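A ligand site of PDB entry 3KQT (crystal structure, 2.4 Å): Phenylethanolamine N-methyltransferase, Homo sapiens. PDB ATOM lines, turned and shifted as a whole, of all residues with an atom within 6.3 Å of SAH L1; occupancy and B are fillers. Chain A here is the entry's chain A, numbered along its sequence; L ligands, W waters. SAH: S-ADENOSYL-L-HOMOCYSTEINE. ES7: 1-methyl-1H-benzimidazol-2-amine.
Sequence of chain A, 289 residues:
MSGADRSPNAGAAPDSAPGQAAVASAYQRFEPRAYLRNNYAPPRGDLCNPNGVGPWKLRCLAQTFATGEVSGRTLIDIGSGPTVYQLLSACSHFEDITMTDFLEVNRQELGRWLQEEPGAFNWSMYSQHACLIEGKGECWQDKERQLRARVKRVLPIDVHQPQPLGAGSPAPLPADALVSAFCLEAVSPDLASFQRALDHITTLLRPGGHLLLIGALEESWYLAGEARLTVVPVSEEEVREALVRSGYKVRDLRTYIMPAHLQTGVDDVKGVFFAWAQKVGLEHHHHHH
A nitrogen (N) of SAH L1 lies within hydrogen-bond range of the backbone carbonyl oxygen of Ala 181 (2.8 Å). OXT of SAH L1 is in hydrogen-bond range of OH of Tyr 35, 2.5 Å away. The side-chain carboxylate of Asp 158 sits at hydrogen-bond distance from a nitrogen (N6) of SAH L1, at 3.0 Å. The backbone carbonyl oxygen (O) of Gly 79 sits at hydrogen-bond distance from a nitrogen (N) of SAH L1 (2.6 Å). OH of Tyr 40 is in hydrogen-bond range of N09 of ES7 L2 (3.0 Å). The side-chain amide oxygen (OD1) of Asn 106 is in hydrogen-bond range of an oxygen (O3') of SAH L1 (3.0 Å). The side-chain sulfur of Cys 183 lies within hydrogen-bond range of a nitrogen (N3) of SAH L1 (3.5 Å). The backbone carbonyl oxygen of Ser 80 sits close to a nitrogen (N) of SAH L1, 3.2 Å away. OD1 of Asp 101 is in hydrogen-bond range of O3' of SAH L1, at 2.7 Å. A nitrogen (N11) of ES7 L2 is in hydrogen-bond range of the side-chain hydroxyl of Tyr 35 (2.7 Å). O of SAH L1 lies within hydrogen-bond range of OH of Tyr 85 (2.9 Å). The side-chain hydroxyl (OH) of Tyr 40 is in hydrogen-bond range of an oxygen (OXT) of SAH L1, at 2.5 Å. N1 of SAH L1 is in hydrogen-bond range of N of Val 159 (2.8 Å).
A sulfur (SD) of SAH L1 lies close to the backbone carbonyl oxygen (O) of Phe 182 (3.5 Å). Merely in contact with SAH L1: Gly 81 (3.1 Å), Val 187 (3.3 Å), Phe 102 (3.3 Å), His 160 (3.4 Å), Thr 83 (3.4 Å), Leu 103 (3.5 Å), Tyr 27 (3.7 Å), Gln 86 (3.8 Å), Ile 157 (3.9 Å) and Tyr 222 (3.999 Å). Within 4 Å of SAH L1: Tyr 27, Tyr 35, Tyr 40, Gly 79, Ser 80, Gly 81, Thr 83, Tyr 85, Gln 86, Asp 101, Phe 102, Leu 103, Asn 106, Ile 157, Asp 158, Val 159, His 160, Ala 181, Phe 182, Cys 183, Val 187 and Tyr 222.
The side-chain carboxylate (OD2) of Asp 77 sits at hydrogen-bond distance from the side-chain hydroxyl (OG) of Ser 80 (2.7 Å). OH of Tyr 40 sits at hydrogen-bond distance from OH of Tyr 85, at 3.4 Å. The side-chain carboxylate (OD1) of Asp 158 lies within hydrogen-bond range of the backbone NH (N) of His 160, 2.9 Å away. OE1 of Gln 86 is in hydrogen-bond range of OG1 of Thr 83 (2.6 Å). OH of Tyr 27 sits at hydrogen-bond distance from O of Ala 186 (2.5 Å). N of Gly 79 is in hydrogen-bond range of OG1 of Thr 100 (2.9 Å). The side-chain hydroxyl (OH) of Tyr 222 sits at hydrogen-bond distance from the side-chain hydroxyl (OH) of Tyr 27. The side-chain hydroxyl (OG1) of Thr 83 sits at hydrogen-bond distance from the backbone carbonyl oxygen (O) of Ser 80, 3.3 Å away.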
ATOM      1  N   ALA A  24      17.092   7.348  -1.033  1.00  0.00           N
ATOM      2  CA  ALA A  24      16.454   6.410  -1.953  1.00  0.00           C
ATOM      3  C   ALA A  24      15.681   5.314  -1.223  1.00  0.00           C
ATOM      4  O   ALA A  24      14.592   4.943  -1.655  1.00  0.00           O
ATOM      5  CB  ALA A  24      17.491   5.786  -2.889  1.00  0.00           C
ATOM      6  N   TYR A  27      12.031   5.426  -0.933  1.00  0.00           N
ATOM      7  CA  TYR A  27      11.183   5.039  -2.067  1.00  0.00           C
ATOM      8  C   TYR A  27      10.686   3.591  -2.041  1.00  0.00           C
ATOM      9  O   TYR A  27       9.797   3.225  -2.804  1.00  0.00           O
ATOM     10  CB  TYR A  27      11.838   5.374  -3.413  1.00  0.00           C
ATOM     11  CG  TYR A  27      11.546   6.789  -3.854  1.00  0.00           C
ATOM     12  CD1 TYR A  27      12.498   7.794  -3.697  1.00  0.00           C
ATOM     13  CD2 TYR A  27      10.308   7.132  -4.396  1.00  0.00           C
ATOM     14  CE1 TYR A  27      12.223   9.093  -4.078  1.00  0.00           C
ATOM     15  CE2 TYR A  27      10.029   8.424  -4.770  1.00  0.00           C
ATOM     16  CZ  TYR A  27      10.990   9.401  -4.606  1.00  0.00           C
ATOM     17  OH  TYR A  27      10.723  10.686  -4.981  1.00  0.00           O
ATOM     18  N   PHE A  30       7.084   3.647  -1.008  1.00  0.00           N
ATOM     19  CA  PHE A  30       6.237   4.378  -1.957  1.00  0.00           C
ATOM     20  C   PHE A  30       5.057   3.548  -2.477  1.00  0.00           C
ATOM     21  O   PHE A  30       5.264   2.541  -3.149  1.00  0.00           O
ATOM     22  CB  PHE A  30       7.128   4.805  -3.124  1.00  0.00           C
ATOM     23  CG  PHE A  30       6.433   5.642  -4.163  1.00  0.00           C
ATOM     24  CD1 PHE A  30       6.621   7.010  -4.192  1.00  0.00           C
ATOM     25  CD2 PHE A  30       5.637   5.055  -5.125  1.00  0.00           C
ATOM     26  CE1 PHE A  30       6.005   7.772  -5.162  1.00  0.00           C
ATOM     27  CE2 PHE A  30       5.026   5.811  -6.083  1.00  0.00           C
ATOM     28  CZ  PHE A  30       5.209   7.181  -6.100  1.00  0.00           C
ATOM     29  N   TYR A  35      -0.130   7.581  -4.171  1.00  0.00           N
ATOM     30  CA  TYR A  35       0.441   8.684  -4.918  1.00  0.00           C
ATOM     31  C   TYR A  35      -0.559   9.213  -5.964  1.00  0.00           C
ATOM     32  O   TYR A  35      -0.784  10.420  -6.076  1.00  0.00           O
ATOM     33  CB  TYR A  35       1.771   8.271  -5.582  1.00  0.00           C
ATOM     34  CG  TYR A  35       2.344   9.354  -6.475  1.00  0.00           C
ATOM     35  CD1 TYR A  35       2.978  10.476  -5.947  1.00  0.00           C
ATOM     36  CD2 TYR A  35       2.236   9.261  -7.867  1.00  0.00           C
ATOM     37  CE1 TYR A  35       3.490  11.468  -6.780  1.00  0.00           C
ATOM     38  CE2 TYR A  35       2.756  10.238  -8.695  1.00  0.00           C
ATOM     39  CZ  TYR A  35       3.371  11.342  -8.149  1.00  0.00           C
ATOM     40  OH  TYR A  35       3.870  12.313  -8.978  1.00  0.00           O
ATOM     41  N   ASN A  39      -2.495  13.002  -6.040  1.00  0.00           N
ATOM     42  CA  ASN A  39      -2.101  13.976  -7.045  1.00  0.00           C
ATOM     43  C   ASN A  39      -2.954  13.996  -8.312  1.00  0.00           C
ATOM     44  O   ASN A  39      -2.943  14.981  -9.042  1.00  0.00           O
ATOM     45  CB  ASN A  39      -0.623  13.810  -7.415  1.00  0.00           C
ATOM     46  CG  ASN A  39       0.301  14.007  -6.233  1.00  0.00           C
ATOM     47  OD1 ASN A  39       0.522  15.125  -5.788  1.00  0.00           O
ATOM     48  ND2 ASN A  39       0.829  12.910  -5.708  1.00  0.00           N
ATOM     49  N   TYR A  40      -3.694  12.931  -8.567  1.00  0.00           N
ATOM     50  CA  TYR A  40      -4.413  12.818  -9.835  1.00  0.00           C
ATOM     51  C   TYR A  40      -5.886  12.446  -9.662  1.00  0.00           C
ATOM     52  O   TYR A  40      -6.554  12.108 -10.638  1.00  0.00           O
ATOM     53  CB  TYR A  40      -3.676  11.865 -10.766  1.00  0.00           C
ATOM     54  CG  TYR A  40      -2.247  12.324 -10.938  1.00  0.00           C
ATOM     55  CD1 TYR A  40      -1.221  11.751 -10.204  1.00  0.00           C
ATOM     56  CD2 TYR A  40      -1.944  13.387 -11.775  1.00  0.00           C
ATOM     57  CE1 TYR A  40       0.068  12.198 -10.338  1.00  0.00           C
ATOM     58  CE2 TYR A  40      -0.661  13.826 -11.918  1.00  0.00           C
ATOM     59  CZ  TYR A  40       0.349  13.231 -11.198  1.00  0.00           C
ATOM     60  OH  TYR A  40       1.626  13.691 -11.354  1.00  0.00           O
ATOM     61  N   ASP A  77      10.470   8.747 -21.597  1.00  0.00           N
ATOM     62  CA  ASP A  77       9.881   9.415 -20.440  1.00  0.00           C
ATOM     63  C   ASP A  77      10.662   8.996 -19.210  1.00  0.00           C
ATOM     64  O   ASP A  77      10.782   7.802 -18.921  1.00  0.00           O
ATOM     65  CB  ASP A  77       8.407   9.020 -20.289  1.00  0.00           C
ATOM     66  CG  ASP A  77       7.719   9.780 -19.180  1.00  0.00           C
ATOM     67  OD1 ASP A  77       8.072  10.959 -18.947  1.00  0.00           O
ATOM     68  OD2 ASP A  77       6.812   9.222 -18.541  1.00  0.00           O
ATOM     69  N   ILE A  78      11.185   9.977 -18.491  1.00  0.00           N
ATOM     70  CA  ILE A  78      12.071   9.746 -17.342  1.00  0.00           C
ATOM     71  C   ILE A  78      11.335   9.782 -16.012  1.00  0.00           C
ATOM     72  O   ILE A  78      10.755  10.812 -15.651  1.00  0.00           O
ATOM     73  CB  ILE A  78      13.156  10.839 -17.257  1.00  0.00           C
ATOM     74  CG1 ILE A  78      13.883  11.009 -18.591  1.00  0.00           C
ATOM     75  CG2 ILE A  78      14.100  10.555 -16.115  1.00  0.00           C
ATOM     76  CD1 ILE A  78      14.537   9.743 -19.087  1.00  0.00           C
ATOM     77  N   GLY A  79      11.380   8.697 -15.259  1.00  0.00           N
ATOM     78  CA  GLY A  79      10.726   8.656 -13.961  1.00  0.00           C
ATOM     79  C   GLY A  79       9.213   8.776 -14.104  1.00  0.00           C
ATOM     80  O   GLY A  79       8.569   9.582 -13.419  1.00  0.00           O
ATOM     81  N   SER A  80       8.655   7.952 -14.983  1.00  0.00           N
ATOM     82  CA  SER A  80       7.229   7.976 -15.288  1.00  0.00           C
ATOM     83  C   SER A  80       6.344   7.768 -14.063  1.00  0.00           C
ATOM     84  O   SER A  80       5.201   8.223 -14.030  1.00  0.00           O
ATOM     85  CB  SER A  80       6.922   6.875 -16.301  1.00  0.00           C
ATOM     86  OG  SER A  80       7.748   6.993 -17.448  1.00  0.00           O
ATOM     87  N   GLY A  81       6.863   7.061 -13.074  1.00  0.00           N
ATOM     88  CA  GLY A  81       6.033   6.633 -11.966  1.00  0.00           C
ATOM     89  C   GLY A  81       4.865   5.815 -12.512  1.00  0.00           C
ATOM     90  O   GLY A  81       5.016   5.062 -13.465  1.00  0.00           O
ATOM     91  N   PRO A  82       3.691   5.968 -11.895  1.00  0.00           N
ATOM     92  CA  PRO A  82       2.494   5.253 -12.332  1.00  0.00           C
ATOM     93  C   PRO A  82       1.599   6.129 -13.203  1.00  0.00           C
ATOM     94  O   PRO A  82       0.397   5.898 -13.232  1.00  0.00           O
ATOM     95  CB  PRO A  82       1.761   4.984 -11.007  1.00  0.00           C
ATOM     96  CG  PRO A  82       2.449   5.895  -9.958  1.00  0.00           C
ATOM     97  CD  PRO A  82       3.418   6.757 -10.681  1.00  0.00           C
ATOM     98  N   THR A  83       2.165   7.132 -13.870  1.00  0.00           N
ATOM     99  CA  THR A  83       1.330   8.097 -14.588  1.00  0.00           C
ATOM    100  C   THR A  83       1.636   8.149 -16.084  1.00  0.00           C
ATOM    101  O   THR A  83       2.763   7.901 -16.508  1.00  0.00           O
ATOM    102  CB  THR A  83       1.409   9.521 -13.961  1.00  0.00           C
ATOM    103  OG1 THR A  83       2.570  10.213 -14.433  1.00  0.00           O
ATOM    104  CG2 THR A  83       1.426   9.451 -12.445  1.00  0.00           C
ATOM    105  N   TYR A  85      -0.236  10.737 -18.102  1.00  0.00           N
ATOM    106  CA  TYR A  85      -0.794  12.002 -18.589  1.00  0.00           C
ATOM    107  C   TYR A  85       0.278  12.811 -19.296  1.00  0.00           C
ATOM    108  O   TYR A  85      -0.018  13.595 -20.196  1.00  0.00           O
ATOM    109  CB  TYR A  85      -1.360  12.847 -17.433  1.00  0.00           C
ATOM    110  CG  TYR A  85      -0.266  13.427 -16.565  1.00  0.00           C
ATOM    111  CD1 TYR A  85       0.245  14.697 -16.833  1.00  0.00           C
ATOM    112  CD2 TYR A  85       0.274  12.712 -15.503  1.00  0.00           C
ATOM    113  CE1 TYR A  85       1.268  15.237 -16.049  1.00  0.00           C
ATOM    114  CE2 TYR A  85       1.297  13.238 -14.718  1.00  0.00           C
ATOM    115  CZ  TYR A  85       1.783  14.500 -15.004  1.00  0.00           C
ATOM    116  OH  TYR A  85       2.793  15.010 -14.240  1.00  0.00           O
ATOM    117  N   GLN A  86       1.531  12.619 -18.882  1.00  0.00           N
ATOM    118  CA  GLN A  86       2.638  13.399 -19.429  1.00  0.00           C
ATOM    119  C   GLN A  86       2.954  13.057 -20.876  1.00  0.00           C
ATOM    120  O   GLN A  86       3.716  13.748 -21.535  1.00  0.00           O
ATOM    121  CB  GLN A  86       3.894  13.277 -18.550  1.00  0.00           C
ATOM    122  CG  GLN A  86       4.478  11.864 -18.427  1.00  0.00           C
ATOM    123  CD  GLN A  86       3.884  11.075 -17.278  1.00  0.00           C
ATOM    124  OE1 GLN A  86       2.801  11.392 -16.785  1.00  0.00           O
ATOM    125  NE2 GLN A  86       4.614  10.041 -16.829  1.00  0.00           N
ATOM    126  N   THR A 100       9.819   4.777 -18.156  1.00  0.00           N
ATOM    127  CA  THR A 100      10.796   4.342 -17.178  1.00  0.00           C
ATOM    128  C   THR A 100      10.372   4.638 -15.737  1.00  0.00           C
ATOM    129  O   THR A 100       9.635   5.579 -15.488  1.00  0.00           O
ATOM    130  CB  THR A 100      12.150   5.047 -17.404  1.00  0.00           C
ATOM    131  OG1 THR A 100      12.043   6.430 -17.016  1.00  0.00           O
ATOM    132  CG2 THR A 100      12.555   4.962 -18.877  1.00  0.00           C
ATOM    133  N   ASP A 101      10.839   3.822 -14.801  1.00  0.00           N
ATOM    134  CA  ASP A 101      10.854   4.210 -13.399  1.00  0.00           C
ATOM    135  C   ASP A 101      11.824   3.378 -12.569  1.00  0.00           C
ATOM    136  O   ASP A 101      12.211   2.277 -12.942  1.00  0.00           O
ATOM    137  CB  ASP A 101       9.469   4.154 -12.757  1.00  0.00           C
ATOM    138  CG  ASP A 101       9.382   5.016 -11.517  1.00  0.00           C
ATOM    139  OD1 ASP A 101       9.424   6.259 -11.657  1.00  0.00           O
ATOM    140  OD2 ASP A 101       9.275   4.467 -10.393  1.00  0.00           O
ATOM    141  N   PHE A 102      12.186   3.929 -11.415  1.00  0.00           N
ATOM    142  CA  PHE A 102      13.103   3.271 -10.495  1.00  0.00           C
ATOM    143  C   PHE A 102      12.435   2.073  -9.823  1.00  0.00           C
ATOM    144  O   PHE A 102      13.062   1.043  -9.604  1.00  0.00           O
ATOM    145  CB  PHE A 102      13.552   4.298  -9.455  1.00  0.00           C
ATOM    146  CG  PHE A 102      14.528   3.766  -8.451  1.00  0.00           C
ATOM    147  CD1 PHE A 102      15.851   3.567  -8.796  1.00  0.00           C
ATOM    148  CD2 PHE A 102      14.127   3.501  -7.150  1.00  0.00           C
ATOM    149  CE1 PHE A 102      16.772   3.080  -7.862  1.00  0.00           C
ATOM    150  CE2 PHE A 102      15.042   3.016  -6.203  1.00  0.00           C
ATOM    151  CZ  PHE A 102      16.361   2.815  -6.566  1.00  0.00           C
ATOM    152  N   LEU A 103      11.149   2.218  -9.509  1.00  0.00           N
ATOM    153  CA  LEU A 103      10.425   1.215  -8.743  1.00  0.00           C
ATOM    154  C   LEU A 103       9.690   0.195  -9.597  1.00  0.00           C
ATOM    155  O   LEU A 103       8.993   0.535 -10.559  1.00  0.00           O
ATOM    156  CB  LEU A 103       9.426   1.881  -7.794  1.00  0.00           C
ATOM    157  CG  LEU A 103      10.041   2.704  -6.660  1.00  0.00           C
ATOM    158  CD1 LEU A 103       8.958   3.463  -5.909  1.00  0.00           C
ATOM    159  CD2 LEU A 103      10.849   1.811  -5.719  1.00  0.00           C
ATOM    160  N   ASN A 106       5.888   0.717  -9.550  1.00  0.00           N
ATOM    161  CA  ASN A 106       5.416   1.701 -10.523  1.00  0.00           C
ATOM    162  C   ASN A 106       5.315   1.117 -11.928  1.00  0.00           C
ATOM    163  O   ASN A 106       4.339   1.362 -12.649  1.00  0.00           O
ATOM    164  CB  ASN A 106       6.271   2.960 -10.510  1.00  0.00           C
ATOM    165  CG  ASN A 106       5.844   3.914  -9.417  1.00  0.00           C
ATOM    166  OD1 ASN A 106       6.630   4.767  -8.976  1.00  0.00           O
ATOM    167  ND2 ASN A 106       4.607   3.780  -8.948  1.00  0.00           N
ATOM    168  N   ILE A 157      15.176   2.443 -14.244  1.00  0.00           N
ATOM    169  CA  ILE A 157      16.047   3.590 -14.454  1.00  0.00           C
ATOM    170  C   ILE A 157      16.509   4.153 -13.113  1.00  0.00           C
ATOM    171  O   ILE A 157      15.832   3.988 -12.094  1.00  0.00           O
ATOM    172  CB  ILE A 157      15.325   4.673 -15.296  1.00  0.00           C
ATOM    173  CG1 ILE A 157      16.309   5.774 -15.724  1.00  0.00           C
ATOM    174  CG2 ILE A 157      14.135   5.253 -14.530  1.00  0.00           C
ATOM    175  CD1 ILE A 157      15.671   6.886 -16.530  1.00  0.00           C
ATOM    176  N   ASP A 158      17.673   4.787 -13.121  1.00  0.00           N
ATOM    177  CA  ASP A 158      18.200   5.454 -11.941  1.00  0.00           C
ATOM    178  C   ASP A 158      18.996   6.665 -12.414  1.00  0.00           C
ATOM    179  O   ASP A 158      20.109   6.516 -12.926  1.00  0.00           O
ATOM    180  CB  ASP A 158      19.106   4.515 -11.138  1.00  0.00           C
ATOM    181  CG  ASP A 158      19.718   5.189  -9.927  1.00  0.00           C
ATOM    182  OD1 ASP A 158      19.560   6.419  -9.759  1.00  0.00           O
ATOM    183  OD2 ASP A 158      20.373   4.480  -9.133  1.00  0.00           O
ATOM    184  N   VAL A 159      18.420   7.854 -12.250  1.00  0.00           N
ATOM    185  CA  VAL A 159      19.016   9.065 -12.816  1.00  0.00           C
ATOM    186  C   VAL A 159      20.296   9.476 -12.086  1.00  0.00           C
ATOM    187  O   VAL A 159      20.969  10.421 -12.485  1.00  0.00           O
ATOM    188  CB  VAL A 159      18.026  10.246 -12.853  1.00  0.00           C
ATOM    189  CG1 VAL A 159      16.802   9.893 -13.704  1.00  0.00           C
ATOM    190  CG2 VAL A 159      17.619  10.638 -11.446  1.00  0.00           C
ATOM    191  N   HIS A 160      20.634   8.762 -11.017  1.00  0.00           N
ATOM    192  CA  HIS A 160      21.867   9.039 -10.302  1.00  0.00           C
ATOM    193  C   HIS A 160      23.058   8.335 -10.953  1.00  0.00           C
ATOM    194  O   HIS A 160      24.199   8.720 -10.726  1.00  0.00           O
ATOM    195  CB  HIS A 160      21.739   8.651  -8.829  1.00  0.00           C
ATOM    196  CG  HIS A 160      20.714   9.449  -8.086  1.00  0.00           C
ATOM    197  ND1 HIS A 160      20.623  10.821  -8.201  1.00  0.00           N
ATOM    198  CD2 HIS A 160      19.729   9.069  -7.236  1.00  0.00           C
ATOM    199  CE1 HIS A 160      19.620  11.249  -7.455  1.00  0.00           C
ATOM    200  NE2 HIS A 160      19.064  10.210  -6.857  1.00  0.00           N
ATOM    201  N   SER A 180      10.059  14.376 -18.763  1.00  0.00           N
ATOM    202  CA  SER A 180      10.151  13.942 -17.384  1.00  0.00           C
ATOM    203  C   SER A 180       9.365  14.865 -16.489  1.00  0.00           C
ATOM    204  O   SER A 180       9.469  16.094 -16.597  1.00  0.00           O
ATOM    205  CB  SER A 180      11.610  13.896 -16.913  1.00  0.00           C
ATOM    206  OG  SER A 180      11.664  13.548 -15.546  1.00  0.00           O
ATOM    207  N   ALA A 181       8.571  14.288 -15.597  1.00  0.00           N
ATOM    208  CA  ALA A 181       7.691  15.082 -14.763  1.00  0.00           C
ATOM    209  C   ALA A 181       7.786  14.698 -13.295  1.00  0.00           C
ATOM    210  O   ALA A 181       7.549  13.555 -12.928  1.00  0.00           O
ATOM    211  CB  ALA A 181       6.239  14.970 -15.245  1.00  0.00           C
ATOM    212  N   PHE A 182       8.125  15.690 -12.466  1.00  0.00           N
ATOM    213  CA  PHE A 182       8.150  15.528 -11.015  1.00  0.00           C
ATOM    214  C   PHE A 182       9.131  14.449 -10.562  1.00  0.00           C
ATOM    215  O   PHE A 182       8.899  13.796  -9.548  1.00  0.00           O
ATOM    216  CB  PHE A 182       6.761  15.214 -10.480  1.00  0.00           C
ATOM    217  CG  PHE A 182       5.762  16.305 -10.732  1.00  0.00           C
ATOM    218  CD1 PHE A 182       4.691  16.095 -11.581  1.00  0.00           C
ATOM    219  CD2 PHE A 182       5.896  17.534 -10.128  1.00  0.00           C
ATOM    220  CE1 PHE A 182       3.770  17.093 -11.809  1.00  0.00           C
ATOM    221  CE2 PHE A 182       4.984  18.546 -10.353  1.00  0.00           C
ATOM    222  CZ  PHE A 182       3.913  18.321 -11.201  1.00  0.00           C
ATOM    223  N   CYS A 183      10.215  14.282 -11.290  1.00  0.00           N
ATOM    224  CA  CYS A 183      11.180  13.250 -10.944  1.00  0.00           C
ATOM    225  C   CYS A 183      12.458  13.817 -10.302  1.00  0.00           C
ATOM    226  O   CYS A 183      12.774  13.531  -9.141  1.00  0.00           O
ATOM    227  CB  CYS A 183      11.536  12.408 -12.168  1.00  0.00           C
ATOM    228  SG  CYS A 183      12.697  11.077 -11.814  1.00  0.00           S
ATOM    229  N   LEU A 184      13.182  14.613 -11.070  1.00  0.00           N
ATOM    230  CA  LEU A 184      14.515  15.041 -10.686  1.00  0.00           C
ATOM    231  C   LEU A 184      14.571  15.689  -9.301  1.00  0.00           C
ATOM    232  O   LEU A 184      15.344  15.278  -8.453  1.00  0.00           O
ATOM    233  CB  LEU A 184      15.119  15.980 -11.737  1.00  0.00           C
ATOM    234  CG  LEU A 184      15.296  15.405 -13.146  1.00  0.00           C
ATOM    235  CD1 LEU A 184      16.413  16.141 -13.855  1.00  0.00           C
ATOM    236  CD2 LEU A 184      15.587  13.912 -13.105  1.00  0.00           C
ATOM    237  N   ALA A 186      12.462  15.447  -7.024  1.00  0.00           N
ATOM    238  CA  ALA A 186      11.877  14.528  -6.060  1.00  0.00           C
ATOM    239  C   ALA A 186      12.794  13.352  -5.681  1.00  0.00           C
ATOM    240  O   ALA A 186      12.432  12.556  -4.814  1.00  0.00           O
ATOM    241  CB  ALA A 186      10.540  13.989  -6.575  1.00  0.00           C
ATOM    242  N   VAL A 187      13.945  13.224  -6.342  1.00  0.00           N
ATOM    243  CA  VAL A 187      14.894  12.156  -6.007  1.00  0.00           C
ATOM    244  C   VAL A 187      16.289  12.698  -5.662  1.00  0.00           C
ATOM    245  O   VAL A 187      17.217  11.928  -5.424  1.00  0.00           O
ATOM    246  CB  VAL A 187      15.040  11.137  -7.162  1.00  0.00           C
ATOM    247  CG1 VAL A 187      13.694  10.528  -7.517  1.00  0.00           C
ATOM    248  CG2 VAL A 187      15.672  11.789  -8.389  1.00  0.00           C
ATOM    249  N   TYR A 222       6.740  15.149   0.164  1.00  0.00           N
ATOM    250  CA  TYR A 222       5.394  14.692  -0.167  1.00  0.00           C
ATOM    251  C   TYR A 222       5.176  13.281   0.324  1.00  0.00           C
ATOM    252  O   TYR A 222       6.130  12.570   0.670  1.00  0.00           O
ATOM    253  CB  TYR A 222       5.127  14.781  -1.669  1.00  0.00           C
ATOM    254  CG  TYR A 222       5.893  13.787  -2.496  1.00  0.00           C
ATOM    255  CD1 TYR A 222       5.244  12.665  -3.016  1.00  0.00           C
ATOM    256  CD2 TYR A 222       7.240  13.948  -2.775  1.00  0.00           C
ATOM    257  CE1 TYR A 222       5.919  11.743  -3.791  1.00  0.00           C
ATOM    258  CE2 TYR A 222       7.930  13.025  -3.559  1.00  0.00           C
ATOM    259  CZ  TYR A 222       7.263  11.926  -4.066  1.00  0.00           C
ATOM    260  OH  TYR A 222       7.905  11.006  -4.842  1.00  0.00           O
HETATM  261  N   SAH L   1       6.420  11.106 -13.646  1.00  0.00           N
HETATM  262  CA  SAH L   1       5.401  10.849 -12.629  1.00  0.00           C
HETATM  263  CB  SAH L   1       6.065  10.364 -11.314  1.00  0.00           C
HETATM  264  CG  SAH L   1       6.462  11.546 -10.400  1.00  0.00           C
HETATM  265  SD  SAH L   1       6.979  10.941  -8.748  1.00  0.00           S
HETATM  266  C   SAH L   1       4.559  12.112 -12.394  1.00  0.00           C
HETATM  267  O   SAH L   1       4.494  12.941 -13.245  1.00  0.00           O
HETATM  268  OXT SAH L   1       3.529  12.025 -11.471  1.00  0.00           O
HETATM  269  C5' SAH L   1       8.785  10.733  -8.733  1.00  0.00           C
HETATM  270  C4' SAH L   1       9.196   9.419  -9.416  1.00  0.00           C
HETATM  271  O4' SAH L   1      10.650   9.247  -9.476  1.00  0.00           O
HETATM  272  C3' SAH L   1       8.616   8.160  -8.743  1.00  0.00           C
HETATM  273  O3' SAH L   1       7.964   7.395  -9.728  1.00  0.00           O
HETATM  274  C2' SAH L   1       9.872   7.460  -8.288  1.00  0.00           C
HETATM  275  O2' SAH L   1       9.788   6.080  -8.035  1.00  0.00           O
HETATM  276  C1' SAH L   1      10.871   7.804  -9.379  1.00  0.00           C
HETATM  277  N9  SAH L   1      12.192   7.572  -8.827  1.00  0.00           N
HETATM  278  C8  SAH L   1      12.511   7.369  -7.390  1.00  0.00           C
HETATM  279  N7  SAH L   1      13.958   7.247  -7.293  1.00  0.00           N
HETATM  280  C5  SAH L   1      14.535   7.387  -8.639  1.00  0.00           C
HETATM  281  C6  SAH L   1      15.955   7.354  -9.145  1.00  0.00           C
HETATM  282  N6  SAH L   1      17.064   7.179  -8.212  1.00  0.00           N
HETATM  283  N1  SAH L   1      16.214   7.528 -10.566  1.00  0.00           N
HETATM  284  C2  SAH L   1      15.077   7.743 -11.532  1.00  0.00           C
HETATM  285  N3  SAH L   1      13.672   7.775 -11.035  1.00  0.00           N
HETATM  286  C4  SAH L   1      13.416   7.602  -9.597  1.00  0.00           C
HETATM  287  C10 ES7 L   2       3.259  15.740  -8.204  1.00  0.00           C
HETATM  288  C01 ES7 L   2       4.158  17.674  -6.759  1.00  0.00           C
HETATM  289  N02 ES7 L   2       3.178  17.029  -7.660  1.00  0.00           N
HETATM  290  C03 ES7 L   2       2.011  17.609  -8.139  1.00  0.00           C
HETATM  291  C04 ES7 L   2       1.415  18.912  -7.910  1.00  0.00           C
HETATM  292  C05 ES7 L   2       0.153  19.262  -8.541  1.00  0.00           C
HETATM  293  C06 ES7 L   2      -0.501  18.302  -9.403  1.00  0.00           C
HETATM  294  C07 ES7 L   2       0.092  17.007  -9.627  1.00  0.00           C
HETATM  295  C08 ES7 L   2       1.354  16.657  -8.995  1.00  0.00           C
HETATM  296  N09 ES7 L   2       2.116  15.534  -9.040  1.00  0.00           N
HETATM  297  N11 ES7 L   2       4.322  14.801  -7.970  1.00  0.00           N
HETATM  298  O   HOH W   1      15.982   6.396  -5.486  1.00  0.00           O
